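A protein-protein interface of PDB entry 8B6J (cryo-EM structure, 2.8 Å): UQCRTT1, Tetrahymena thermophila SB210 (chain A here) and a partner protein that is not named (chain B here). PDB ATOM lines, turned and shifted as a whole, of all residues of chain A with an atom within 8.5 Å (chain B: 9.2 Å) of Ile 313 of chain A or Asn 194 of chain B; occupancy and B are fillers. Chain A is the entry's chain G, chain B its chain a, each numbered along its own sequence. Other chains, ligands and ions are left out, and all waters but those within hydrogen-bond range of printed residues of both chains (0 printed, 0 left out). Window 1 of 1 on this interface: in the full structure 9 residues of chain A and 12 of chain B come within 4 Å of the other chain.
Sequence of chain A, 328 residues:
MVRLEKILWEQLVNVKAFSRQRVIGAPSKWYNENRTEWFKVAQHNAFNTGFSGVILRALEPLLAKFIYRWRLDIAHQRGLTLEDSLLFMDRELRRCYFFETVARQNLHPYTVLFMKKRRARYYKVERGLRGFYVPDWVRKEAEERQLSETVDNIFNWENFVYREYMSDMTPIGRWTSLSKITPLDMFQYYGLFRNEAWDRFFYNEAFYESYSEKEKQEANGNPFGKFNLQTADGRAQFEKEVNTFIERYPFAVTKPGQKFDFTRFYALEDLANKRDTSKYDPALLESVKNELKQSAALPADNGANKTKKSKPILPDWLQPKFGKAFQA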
ATOM      1  N   LYS A 308     -14.077  -8.205  -4.219  1.00  0.00           N
ATOM      2  CA  LYS A 308     -14.911  -9.341  -4.586  1.00  0.00           C
ATOM      3  C   LYS A 308     -16.194  -8.874  -5.261  1.00  0.00           C
ATOM      4  O   LYS A 308     -16.777  -7.852  -4.892  1.00  0.00           O
ATOM      5  CB  LYS A 308     -15.247 -10.178  -3.352  1.00  0.00           C
ATOM      6  CG  LYS A 308     -14.075 -10.976  -2.813  1.00  0.00           C
ATOM      7  CD  LYS A 308     -14.534 -12.032  -1.822  1.00  0.00           C
ATOM      8  CE  LYS A 308     -13.361 -12.826  -1.271  1.00  0.00           C
ATOM      9  NZ  LYS A 308     -13.798 -13.864  -0.298  1.00  0.00           N
ATOM     10  N   LYS A 309     -16.630  -9.636  -6.261  1.00  0.00           N
ATOM     11  CA  LYS A 309     -17.862  -9.349  -6.980  1.00  0.00           C
ATOM     12  C   LYS A 309     -19.029 -10.033  -6.278  1.00  0.00           C
ATOM     13  O   LYS A 309     -18.982 -11.237  -6.007  1.00  0.00           O
ATOM     14  CB  LYS A 309     -17.757  -9.824  -8.429  1.00  0.00           C
ATOM     15  CG  LYS A 309     -18.987  -9.539  -9.271  1.00  0.00           C
ATOM     16  CD  LYS A 309     -18.755  -9.906 -10.725  1.00  0.00           C
ATOM     17  CE  LYS A 309     -19.995  -9.659 -11.563  1.00  0.00           C
ATOM     18  NZ  LYS A 309     -19.756  -9.938 -13.004  1.00  0.00           N
ATOM     19  N   SER A 310     -20.072  -9.261  -5.988  1.00  0.00           N
ATOM     20  CA  SER A 310     -21.214  -9.794  -5.259  1.00  0.00           C
ATOM     21  C   SER A 310     -21.957 -10.828  -6.094  1.00  0.00           C
ATOM     22  O   SER A 310     -22.185 -10.637  -7.292  1.00  0.00           O
ATOM     23  CB  SER A 310     -22.161  -8.663  -4.862  1.00  0.00           C
ATOM     24  OG  SER A 310     -22.608  -7.950  -6.000  1.00  0.00           O
ATOM     25  N   LYS A 311     -22.339 -11.928  -5.450  1.00  0.00           N
ATOM     26  CA  LYS A 311     -23.134 -12.989  -6.067  1.00  0.00           C
ATOM     27  C   LYS A 311     -24.318 -13.286  -5.157  1.00  0.00           C
ATOM     28  O   LYS A 311     -24.364 -14.327  -4.492  1.00  0.00           O
ATOM     29  CB  LYS A 311     -22.293 -14.244  -6.303  1.00  0.00           C
ATOM     30  CG  LYS A 311     -21.183 -14.055  -7.320  1.00  0.00           C
ATOM     31  CD  LYS A 311     -20.461 -15.360  -7.606  1.00  0.00           C
ATOM     32  CE  LYS A 311     -19.371 -15.172  -8.646  1.00  0.00           C
ATOM     33  NZ  LYS A 311     -18.642 -16.438  -8.922  1.00  0.00           N
ATOM     34  N   PRO A 312     -25.298 -12.385  -5.107  1.00  0.00           N
ATOM     35  CA  PRO A 312     -26.386 -12.537  -4.135  1.00  0.00           C
ATOM     36  C   PRO A 312     -27.186 -13.812  -4.352  1.00  0.00           C
ATOM     37  O   PRO A 312     -27.364 -14.282  -5.477  1.00  0.00           O
ATOM     38  CB  PRO A 312     -27.247 -11.288  -4.367  1.00  0.00           C
ATOM     39  CG  PRO A 312     -26.905 -10.833  -5.737  1.00  0.00           C
ATOM     40  CD  PRO A 312     -25.470 -11.188  -5.945  1.00  0.00           C
ATOM     41  N   ILE A 313     -27.671 -14.366  -3.241  1.00  0.00           N
ATOM     42  CA  ILE A 313     -28.486 -15.571  -3.236  1.00  0.00           C
ATOM     43  C   ILE A 313     -29.737 -15.288  -2.414  1.00  0.00           C
ATOM     44  O   ILE A 313     -29.760 -14.394  -1.564  1.00  0.00           O
ATOM     45  CB  ILE A 313     -27.720 -16.788  -2.668  1.00  0.00           C
ATOM     46  CG1 ILE A 313     -26.428 -17.009  -3.458  1.00  0.00           C
ATOM     47  CG2 ILE A 313     -28.589 -18.037  -2.707  1.00  0.00           C
ATOM     48  CD1 ILE A 313     -25.514 -18.063  -2.868  1.00  0.00           C
ATOM     49  N   LEU A 314     -30.785 -16.057  -2.682  1.00  0.00           N
ATOM     50  CA  LEU A 314     -32.057 -15.821  -2.020  1.00  0.00           C
ATOM     51  C   LEU A 314     -31.915 -16.031  -0.513  1.00  0.00           C
ATOM     52  O   LEU A 314     -31.187 -16.931  -0.078  1.00  0.00           O
ATOM     53  CB  LEU A 314     -33.132 -16.754  -2.578  1.00  0.00           C
ATOM     54  CG  LEU A 314     -33.523 -16.524  -4.039  1.00  0.00           C
ATOM     55  CD1 LEU A 314     -34.499 -17.590  -4.498  1.00  0.00           C
ATOM     56  CD2 LEU A 314     -34.118 -15.139  -4.230  1.00  0.00           C
ATOM     57  N   PRO A 315     -32.586 -15.225   0.310  1.00  0.00           N
ATOM     58  CA  PRO A 315     -32.525 -15.435   1.762  1.00  0.00           C
ATOM     59  C   PRO A 315     -33.024 -16.819   2.148  1.00  0.00           C
ATOM     60  O   PRO A 315     -33.658 -17.533   1.368  1.00  0.00           O
ATOM     61  CB  PRO A 315     -33.434 -14.338   2.322  1.00  0.00           C
ATOM     62  CG  PRO A 315     -33.459 -13.293   1.274  1.00  0.00           C
ATOM     63  CD  PRO A 315     -33.345 -14.011  -0.034  1.00  0.00           C
ATOM     64  N   ASP A 316     -32.724 -17.197   3.392  1.00  0.00           N
ATOM     65  CA  ASP A 316     -33.106 -18.521   3.871  1.00  0.00           C
ATOM     66  C   ASP A 316     -34.621 -18.685   3.908  1.00  0.00           C
ATOM     67  O   ASP A 316     -35.147 -19.738   3.529  1.00  0.00           O
ATOM     68  CB  ASP A 316     -32.508 -18.766   5.256  1.00  0.00           C
ATOM     69  CG  ASP A 316     -30.998 -18.652   5.265  1.00  0.00           C
ATOM     70  OD1 ASP A 316     -30.428 -18.231   4.237  1.00  0.00           O
ATOM     71  OD2 ASP A 316     -30.379 -18.985   6.298  1.00  0.00           O
ATOM     72  N   LEU A 318     -36.803 -17.592   2.031  1.00  0.00           N
ATOM     73  CA  LEU A 318     -37.348 -17.775   0.694  1.00  0.00           C
ATOM     74  C   LEU A 318     -36.858 -19.059   0.038  1.00  0.00           C
ATOM     75  O   LEU A 318     -37.033 -19.230  -1.172  1.00  0.00           O
ATOM     76  CB  LEU A 318     -36.997 -16.577  -0.192  1.00  0.00           C
ATOM     77  CG  LEU A 318     -37.697 -15.250   0.110  1.00  0.00           C
ATOM     78  CD1 LEU A 318     -37.282 -14.193  -0.893  1.00  0.00           C
ATOM     79  CD2 LEU A 318     -39.202 -15.414   0.102  1.00  0.00           C
ATOM     80  N   GLN A 319     -36.250 -19.959   0.802  1.00  0.00           N
ATOM     81  CA  GLN A 319     -35.719 -21.215   0.307  1.00  0.00           C
ATOM     82  C   GLN A 319     -36.381 -22.384   1.026  1.00  0.00           C
ATOM     83  O   GLN A 319     -36.863 -22.237   2.156  1.00  0.00           O
ATOM     84  CB  GLN A 319     -34.199 -21.281   0.507  1.00  0.00           C
ATOM     85  CG  GLN A 319     -33.424 -20.281  -0.329  1.00  0.00           C
ATOM     86  CD  GLN A 319     -31.948 -20.262   0.006  1.00  0.00           C
ATOM     87  OE1 GLN A 319     -31.476 -21.048   0.827  1.00  0.00           O
ATOM     88  NE2 GLN A 319     -31.210 -19.359  -0.627  1.00  0.00           N
ATOM     89  N   ASN B 187     -12.529 -13.807   4.255  1.00  0.00           N
ATOM     90  CA  ASN B 187     -13.382 -14.150   3.124  1.00  0.00           C
ATOM     91  C   ASN B 187     -14.852 -14.108   3.515  1.00  0.00           C
ATOM     92  O   ASN B 187     -15.694 -13.651   2.737  1.00  0.00           O
ATOM     93  CB  ASN B 187     -13.008 -15.529   2.582  1.00  0.00           C
ATOM     94  CG  ASN B 187     -11.697 -15.518   1.823  1.00  0.00           C
ATOM     95  OD1 ASN B 187     -10.940 -14.548   1.882  1.00  0.00           O
ATOM     96  ND2 ASN B 187     -11.420 -16.598   1.104  1.00  0.00           N
ATOM     97  N   ASN B 188     -15.183 -14.593   4.713  1.00  0.00           N
ATOM     98  CA  ASN B 188     -16.565 -14.517   5.180  1.00  0.00           C
ATOM     99  C   ASN B 188     -17.021 -13.069   5.314  1.00  0.00           C
ATOM    100  O   ASN B 188     -18.144 -12.724   4.926  1.00  0.00           O
ATOM    101  CB  ASN B 188     -16.706 -15.246   6.515  1.00  0.00           C
ATOM    102  CG  ASN B 188     -18.036 -14.978   7.186  1.00  0.00           C
ATOM    103  OD1 ASN B 188     -18.153 -14.089   8.028  1.00  0.00           O
ATOM    104  ND2 ASN B 188     -19.052 -15.748   6.813  1.00  0.00           N
ATOM    105  N   ALA B 189     -16.163 -12.209   5.862  1.00  0.00           N
ATOM    106  CA  ALA B 189     -16.519 -10.801   5.990  1.00  0.00           C
ATOM    107  C   ALA B 189     -16.768 -10.173   4.625  1.00  0.00           C
ATOM    108  O   ALA B 189     -17.727  -9.415   4.447  1.00  0.00           O
ATOM    109  CB  ALA B 189     -15.418 -10.046   6.733  1.00  0.00           C
ATOM    110  N   LEU B 190     -15.913 -10.478   3.648  1.00  0.00           N
ATOM    111  CA  LEU B 190     -16.105  -9.926   2.310  1.00  0.00           C
ATOM    112  C   LEU B 190     -17.370 -10.472   1.658  1.00  0.00           C
ATOM    113  O   LEU B 190     -18.095  -9.732   0.984  1.00  0.00           O
ATOM    114  CB  LEU B 190     -14.890 -10.222   1.435  1.00  0.00           C
ATOM    115  CG  LEU B 190     -13.594  -9.479   1.768  1.00  0.00           C
ATOM    116  CD1 LEU B 190     -12.508  -9.863   0.777  1.00  0.00           C
ATOM    117  CD2 LEU B 190     -13.809  -7.973   1.775  1.00  0.00           C
ATOM    118  N   SER B 191     -17.653 -11.762   1.844  1.00  0.00           N
ATOM    119  CA  SER B 191     -18.799 -12.399   1.209  1.00  0.00           C
ATOM    120  C   SER B 191     -20.113 -12.101   1.915  1.00  0.00           C
ATOM    121  O   SER B 191     -21.172 -12.450   1.383  1.00  0.00           O
ATOM    122  CB  SER B 191     -18.587 -13.913   1.156  1.00  0.00           C
ATOM    123  OG  SER B 191     -17.418 -14.239   0.427  1.00  0.00           O
ATOM    124  N   ALA B 192     -20.071 -11.484   3.098  1.00  0.00           N
ATOM    125  CA  ALA B 192     -21.306 -11.110   3.779  1.00  0.00           C
ATOM    126  C   ALA B 192     -22.280 -10.390   2.853  1.00  0.00           C
ATOM    127  O   ALA B 192     -23.494 -10.422   3.086  1.00  0.00           O
ATOM    128  CB  ALA B 192     -20.988 -10.227   4.987  1.00  0.00           C
ATOM    129  N   GLN B 193     -21.776  -9.736   1.804  1.00  0.00           N
ATOM    130  CA  GLN B 193     -22.651  -9.014   0.887  1.00  0.00           C
ATOM    131  C   GLN B 193     -23.540  -9.940   0.067  1.00  0.00           C
ATOM    132  O   GLN B 193     -24.507  -9.469  -0.536  1.00  0.00           O
ATOM    133  CB  GLN B 193     -21.823  -8.143  -0.058  1.00  0.00           C
ATOM    134  CG  GLN B 193     -20.844  -8.921  -0.918  1.00  0.00           C
ATOM    135  CD  GLN B 193     -20.127  -8.043  -1.918  1.00  0.00           C
ATOM    136  OE1 GLN B 193     -20.482  -6.880  -2.103  1.00  0.00           O
ATOM    137  NE2 GLN B 193     -19.113  -8.596  -2.570  1.00  0.00           N
ATOM    138  N   ASN B 194     -23.232 -11.238   0.023  1.00  0.00           N
ATOM    139  CA  ASN B 194     -24.063 -12.159  -0.746  1.00  0.00           C
ATOM    140  C   ASN B 194     -25.489 -12.186  -0.214  1.00  0.00           C
ATOM    141  O   ASN B 194     -26.449 -12.174  -0.991  1.00  0.00           O
ATOM    142  CB  ASN B 194     -23.451 -13.558  -0.720  1.00  0.00           C
ATOM    143  CG  ASN B 194     -22.126 -13.624  -1.447  1.00  0.00           C
ATOM    144  OD1 ASN B 194     -21.536 -12.596  -1.778  1.00  0.00           O
ATOM    145  ND2 ASN B 194     -21.648 -14.836  -1.699  1.00  0.00           N
ATOM    146  N   ASP B 195     -25.650 -12.220   1.105  1.00  0.00           N
ATOM    147  CA  ASP B 195     -26.972 -12.158   1.722  1.00  0.00           C
ATOM    148  C   ASP B 195     -27.354 -10.689   1.834  1.00  0.00           C
ATOM    149  O   ASP B 195     -27.023 -10.006   2.804  1.00  0.00           O
ATOM    150  CB  ASP B 195     -26.971 -12.848   3.080  1.00  0.00           C
ATOM    151  CG  ASP B 195     -28.361 -12.983   3.666  1.00  0.00           C
ATOM    152  OD1 ASP B 195     -29.333 -12.598   2.984  1.00  0.00           O
ATOM    153  OD2 ASP B 195     -28.483 -13.474   4.807  1.00  0.00           O
ATOM    154  N   GLN B 196     -28.064 -10.193   0.818  1.00  0.00           N
ATOM    155  CA  GLN B 196     -28.384  -8.771   0.766  1.00  0.00           C
ATOM    156  C   GLN B 196     -29.218  -8.346   1.967  1.00  0.00           C
ATOM    157  O   GLN B 196     -28.979  -7.284   2.554  1.00  0.00           O
ATOM    158  CB  GLN B 196     -29.113  -8.452  -0.538  1.00  0.00           C
ATOM    159  CG  GLN B 196     -28.275  -8.699  -1.783  1.00  0.00           C
ATOM    160  CD  GLN B 196     -29.042  -8.450  -3.063  1.00  0.00           C
ATOM    161  OE1 GLN B 196     -30.259  -8.614  -3.112  1.00  0.00           O
ATOM    162  NE2 GLN B 196     -28.332  -8.046  -4.109  1.00  0.00           N
ATOM    163  N   GLN B 197     -30.199  -9.163   2.353  1.00  0.00           N
ATOM    164  CA  GLN B 197     -31.024  -8.822   3.506  1.00  0.00           C
ATOM    165  C   GLN B 197     -30.187  -8.745   4.776  1.00  0.00           C
ATOM    166  O   GLN B 197     -30.361  -7.832   5.589  1.00  0.00           O
ATOM    167  CB  GLN B 197     -32.146  -9.846   3.667  1.00  0.00           C
ATOM    168  CG  GLN B 197     -33.137  -9.507   4.767  1.00  0.00           C
ATOM    169  CD  GLN B 197     -34.164 -10.598   4.983  1.00  0.00           C
ATOM    170  OE1 GLN B 197     -35.367 -10.337   5.008  1.00  0.00           O
ATOM    171  NE2 GLN B 197     -33.696 -11.828   5.151  1.00  0.00           N
ATOM    172  N   GLY B 198     -29.272  -9.698   4.966  1.00  0.00           N
ATOM    173  CA  GLY B 198     -28.435  -9.671   6.153  1.00  0.00           C
ATOM    174  C   GLY B 198     -27.524  -8.459   6.197  1.00  0.00           C
ATOM    175  O   GLY B 198     -27.360  -7.826   7.244  1.00  0.00           O
ATOM    176  N   LEU B 199     -26.917  -8.120   5.059  1.00  0.00           N
ATOM    177  CA  LEU B 199     -26.049  -6.950   5.019  1.00  0.00           C
ATOM    178  C   LEU B 199     -26.840  -5.675   5.271  1.00  0.00           C
ATOM    179  O   LEU B 199     -26.351  -4.753   5.933  1.00  0.00           O
ATOM    180  CB  LEU B 199     -25.317  -6.881   3.680  1.00  0.00           C
ATOM    181  CG  LEU B 199     -24.289  -5.755   3.549  1.00  0.00           C
ATOM    182  CD1 LEU B 199     -23.274  -5.808   4.679  1.00  0.00           C
ATOM    183  CD2 LEU B 199     -23.587  -5.831   2.207  1.00  0.00           C
ATOM    184  N   LEU B 200     -28.072  -5.601   4.761  1.00  0.00           N
ATOM    185  CA  LEU B 200     -28.889  -4.424   5.039  1.00  0.00           C
ATOM    186  C   LEU B 200     -29.300  -4.362   6.505  1.00  0.00           C
ATOM    187  O   LEU B 200     -29.409  -3.270   7.072  1.00  0.00           O
ATOM    188  CB  LEU B 200     -30.125  -4.407   4.144  1.00  0.00           C
ATOM    189  CG  LEU B 200     -30.728  -3.008   3.985  1.00  0.00           C
ATOM    190  CD1 LEU B 200     -29.855  -2.151   3.080  1.00  0.00           C
ATOM    191  CD2 LEU B 200     -32.145  -3.076   3.459  1.00  0.00           C
ATOM    192  N   MET B 299     -26.770  -2.494  -9.833  1.00  0.00           N
ATOM    193  CA  MET B 299     -27.379  -3.591  -9.096  1.00  0.00           C
ATOM    194  C   MET B 299     -28.744  -4.016  -9.619  1.00  0.00           C
ATOM    195  O   MET B 299     -29.207  -5.099  -9.249  1.00  0.00           O
ATOM    196  CB  MET B 299     -27.521  -3.222  -7.612  1.00  0.00           C
ATOM    197  CG  MET B 299     -26.196  -3.081  -6.885  1.00  0.00           C
ATOM    198  SD  MET B 299     -26.390  -2.650  -5.147  1.00  0.00           S
ATOM    199  CE  MET B 299     -27.342  -4.043  -4.549  1.00  0.00           C
ATOM    200  N   ASN B 303     -32.360  -2.177  -2.206  1.00  0.00           N
ATOM    201  CA  ASN B 303     -32.643  -2.731  -0.884  1.00  0.00           C
ATOM    202  C   ASN B 303     -32.876  -1.558   0.058  1.00  0.00           C
ATOM    203  O   ASN B 303     -31.946  -0.799   0.342  1.00  0.00           O
ATOM    204  CB  ASN B 303     -31.482  -3.586  -0.375  1.00  0.00           C
ATOM    205  CG  ASN B 303     -30.998  -4.593  -1.392  1.00  0.00           C
ATOM    206  OD1 ASN B 303     -31.253  -5.788  -1.263  1.00  0.00           O
ATOM    207  ND2 ASN B 303     -30.279  -4.120  -2.400  1.00  0.00           N
ATOM    208  N   ILE B 363     -39.742  -8.194  -2.781  1.00  0.00           N
ATOM    209  CA  ILE B 363     -39.629  -8.794  -1.457  1.00  0.00           C
ATOM    210  C   ILE B 363     -39.975  -7.746  -0.412  1.00  0.00           C
ATOM    211  O   ILE B 363     -39.578  -6.583  -0.529  1.00  0.00           O
ATOM    212  CB  ILE B 363     -38.221  -9.365  -1.204  1.00  0.00           C
ATOM    213  CG1 ILE B 363     -37.768 -10.209  -2.396  1.00  0.00           C
ATOM    214  CG2 ILE B 363     -38.211 -10.199   0.070  1.00  0.00           C
ATOM    215  CD1 ILE B 363     -36.423 -10.875  -2.204  1.00  0.00           C
ATOM    216  N   TYR B 380     -38.189  -4.276   5.641  1.00  0.00           N
ATOM    217  CA  TYR B 380     -37.175  -4.323   4.600  1.00  0.00           C
ATOM    218  C   TYR B 380     -37.852  -4.668   3.284  1.00  0.00           C
ATOM    219  O   TYR B 380     -38.471  -5.733   3.163  1.00  0.00           O
ATOM    220  CB  TYR B 380     -36.096  -5.352   4.938  1.00  0.00           C
ATOM    221  CG  TYR B 380     -35.441  -5.978   3.730  1.00  0.00           C
ATOM    222  CD1 TYR B 380     -34.501  -5.281   2.988  1.00  0.00           C
ATOM    223  CD2 TYR B 380     -35.758  -7.269   3.337  1.00  0.00           C
ATOM    224  CE1 TYR B 380     -33.897  -5.849   1.885  1.00  0.00           C
ATOM    225  CE2 TYR B 380     -35.157  -7.847   2.235  1.00  0.00           C
ATOM    226  CZ  TYR B 380     -34.228  -7.131   1.514  1.00  0.00           C
ATOM    227  OH  TYR B 380     -33.627  -7.701   0.416  1.00  0.00           O
ATOM    228  N   TYR B 382     -37.252  -4.979  -1.023  1.00  0.00           N
ATOM    229  CA  TYR B 382     -36.277  -5.188  -2.084  1.00  0.00           C
ATOM    230  C   TYR B 382     -37.029  -5.191  -3.403  1.00  0.00           C
ATOM    231  O   TYR B 382     -37.918  -6.025  -3.608  1.00  0.00           O
ATOM    232  CB  TYR B 382     -35.515  -6.498  -1.893  1.00  0.00           C
ATOM    233  CG  TYR B 382     -34.567  -6.818  -3.021  1.00  0.00           C
ATOM    234  CD1 TYR B 382     -33.380  -6.124  -3.170  1.00  0.00           C
ATOM    235  CD2 TYR B 382     -34.858  -7.819  -3.933  1.00  0.00           C
ATOM    236  CE1 TYR B 382     -32.509  -6.412  -4.197  1.00  0.00           C
ATOM    237  CE2 TYR B 382     -33.994  -8.115  -4.964  1.00  0.00           C
ATOM    238  CZ  TYR B 382     -32.820  -7.409  -5.091  1.00  0.00           C
ATOM    239  OH  TYR B 382     -31.954  -7.698  -6.117  1.00  0.00           O
ATOM    240  N   TRP B 481     -29.734   0.940  -0.190  1.00  0.00           N
ATOM    241  CA  TRP B 481     -28.550   0.393  -0.837  1.00  0.00           C
ATOM    242  C   TRP B 481     -28.906   0.035  -2.272  1.00  0.00           C
ATOM    243  O   TRP B 481     -29.816  -0.767  -2.508  1.00  0.00           O
ATOM    244  CB  TRP B 481     -28.045  -0.834  -0.074  1.00  0.00           C
ATOM    245  CG  TRP B 481     -26.892  -1.530  -0.714  1.00  0.00           C
ATOM    246  CD1 TRP B 481     -25.986  -0.996  -1.579  1.00  0.00           C
ATOM    247  CD2 TRP B 481     -26.523  -2.902  -0.543  1.00  0.00           C
ATOM    248  NE1 TRP B 481     -25.074  -1.949  -1.956  1.00  0.00           N
ATOM    249  CE2 TRP B 481     -25.383  -3.129  -1.334  1.00  0.00           C
ATOM    250  CE3 TRP B 481     -27.048  -3.961   0.203  1.00  0.00           C
ATOM    251  CZ2 TRP B 481     -24.757  -4.369  -1.399  1.00  0.00           C
ATOM    252  CZ3 TRP B 481     -26.425  -5.190   0.136  1.00  0.00           C
ATOM    253  CH2 TRP B 481     -25.293  -5.385  -0.659  1.00  0.00           C
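The backbone carbonyl oxygen of Lys 308 of chain A lies within hydrogen-bond range of the side-chain amide nitrogen of Gln 193 of chain B, 3.4 Å away.
O of Asn 194 of chain B is in hydrogen-bond range of N of Ile 313 of chain A, at 3.4 Å.
O of Asn 187 of chain B is in hydrogen-bond range of OG of Ser 191 of chain B (2.9 Å).
The backbone carbonyl oxygen (O) of Ser 191 of chain B sits close to the side-chain amide oxygen (OD1) of Asn 194 of chain B, at 3.2 Å.
The backbone NH (N) of Tyr 382 of chain B lies within hydrogen-bond range of the backbone carbonyl oxygen (O) of Ile 363 of chain B (2.9 Å).
Asn 187 of chain B touches Lys 308 of chain A (CG to NZ, 3.4 Å).
Lys 308 of chain A touches Leu 190 of chain B.
Lys 308 of chain A touches Ser 191 of chain B.
NE2 of Gln 193 of chain B touches C of Lys 309 of chain A, at 3.98 Å.
Ser 310 of chain A touches Gln 193 of chain B.
OD1 of Asn 194 of chain B touches N of Lys 311 of chain A, at 3.8 Å.
Pro 312 of chain A touches Asn 194 of chain B.
Pro 312 of chain A touches Gln 196 of chain B (CB to NE2, 3.4 Å).
CB of Pro 315 of chain A touches NE2 of Gln 197 of chain B, 3.8 Å away.
Leu 318 of chain A touches Ile 363 of chain B.
Of the printed residues of chain B, Lys 308 of chain A touches Asn 187, Leu 190, Ser 191 and Gln 193.
Of the printed residues of chain B, Ser 310 of chain A touches Gln 193.
Pro 312 of chain A touches just these residues of chain B: Asn 194 (3.2 Å) and Gln 196 (3.4 Å).
Of chain B, only Asn 194 comes within 4 Å of Ile 313 of chain A.
Of the printed residues of chain B, Pro 315 of chain A touches Gln 197 (3.8 Å).
Of the printed residues of chain A, Leu 190 of chain B touches Lys 308 (3.7 Å).
Asn 194 of chain B touches just these residues of chain A: Lys 311 (3.8 Å), Pro 312 (3.2 Å) and Ile 313 (3.4 Å).
The nearest residue of chain B that does not touch Ile 313 of chain A is Asp 195 of chain B (4.9 Å).
The nearest residue of chain A that does not touch Asn 194 of chain B is Ser 310 of chain A (4.5 Å).
The nearest printed residue of chain A that does not touch Ile 363 of chain B is Pro 315 of chain A (4.9 Å).
Of the 11 printed residues of chain A, 8 touch a printed residue of chain B.
Printed residues of chain B that touch a printed residue of chain A: Asn 187, Leu 190, Ser 191, Gln 193, Asn 194, Gln 196, Gln 197 and Ile 363.
Among the printed residues, no Asp or Glu carboxylate lies within 4 Å of a Lys or Arg side-chain nitrogen of the other chain.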
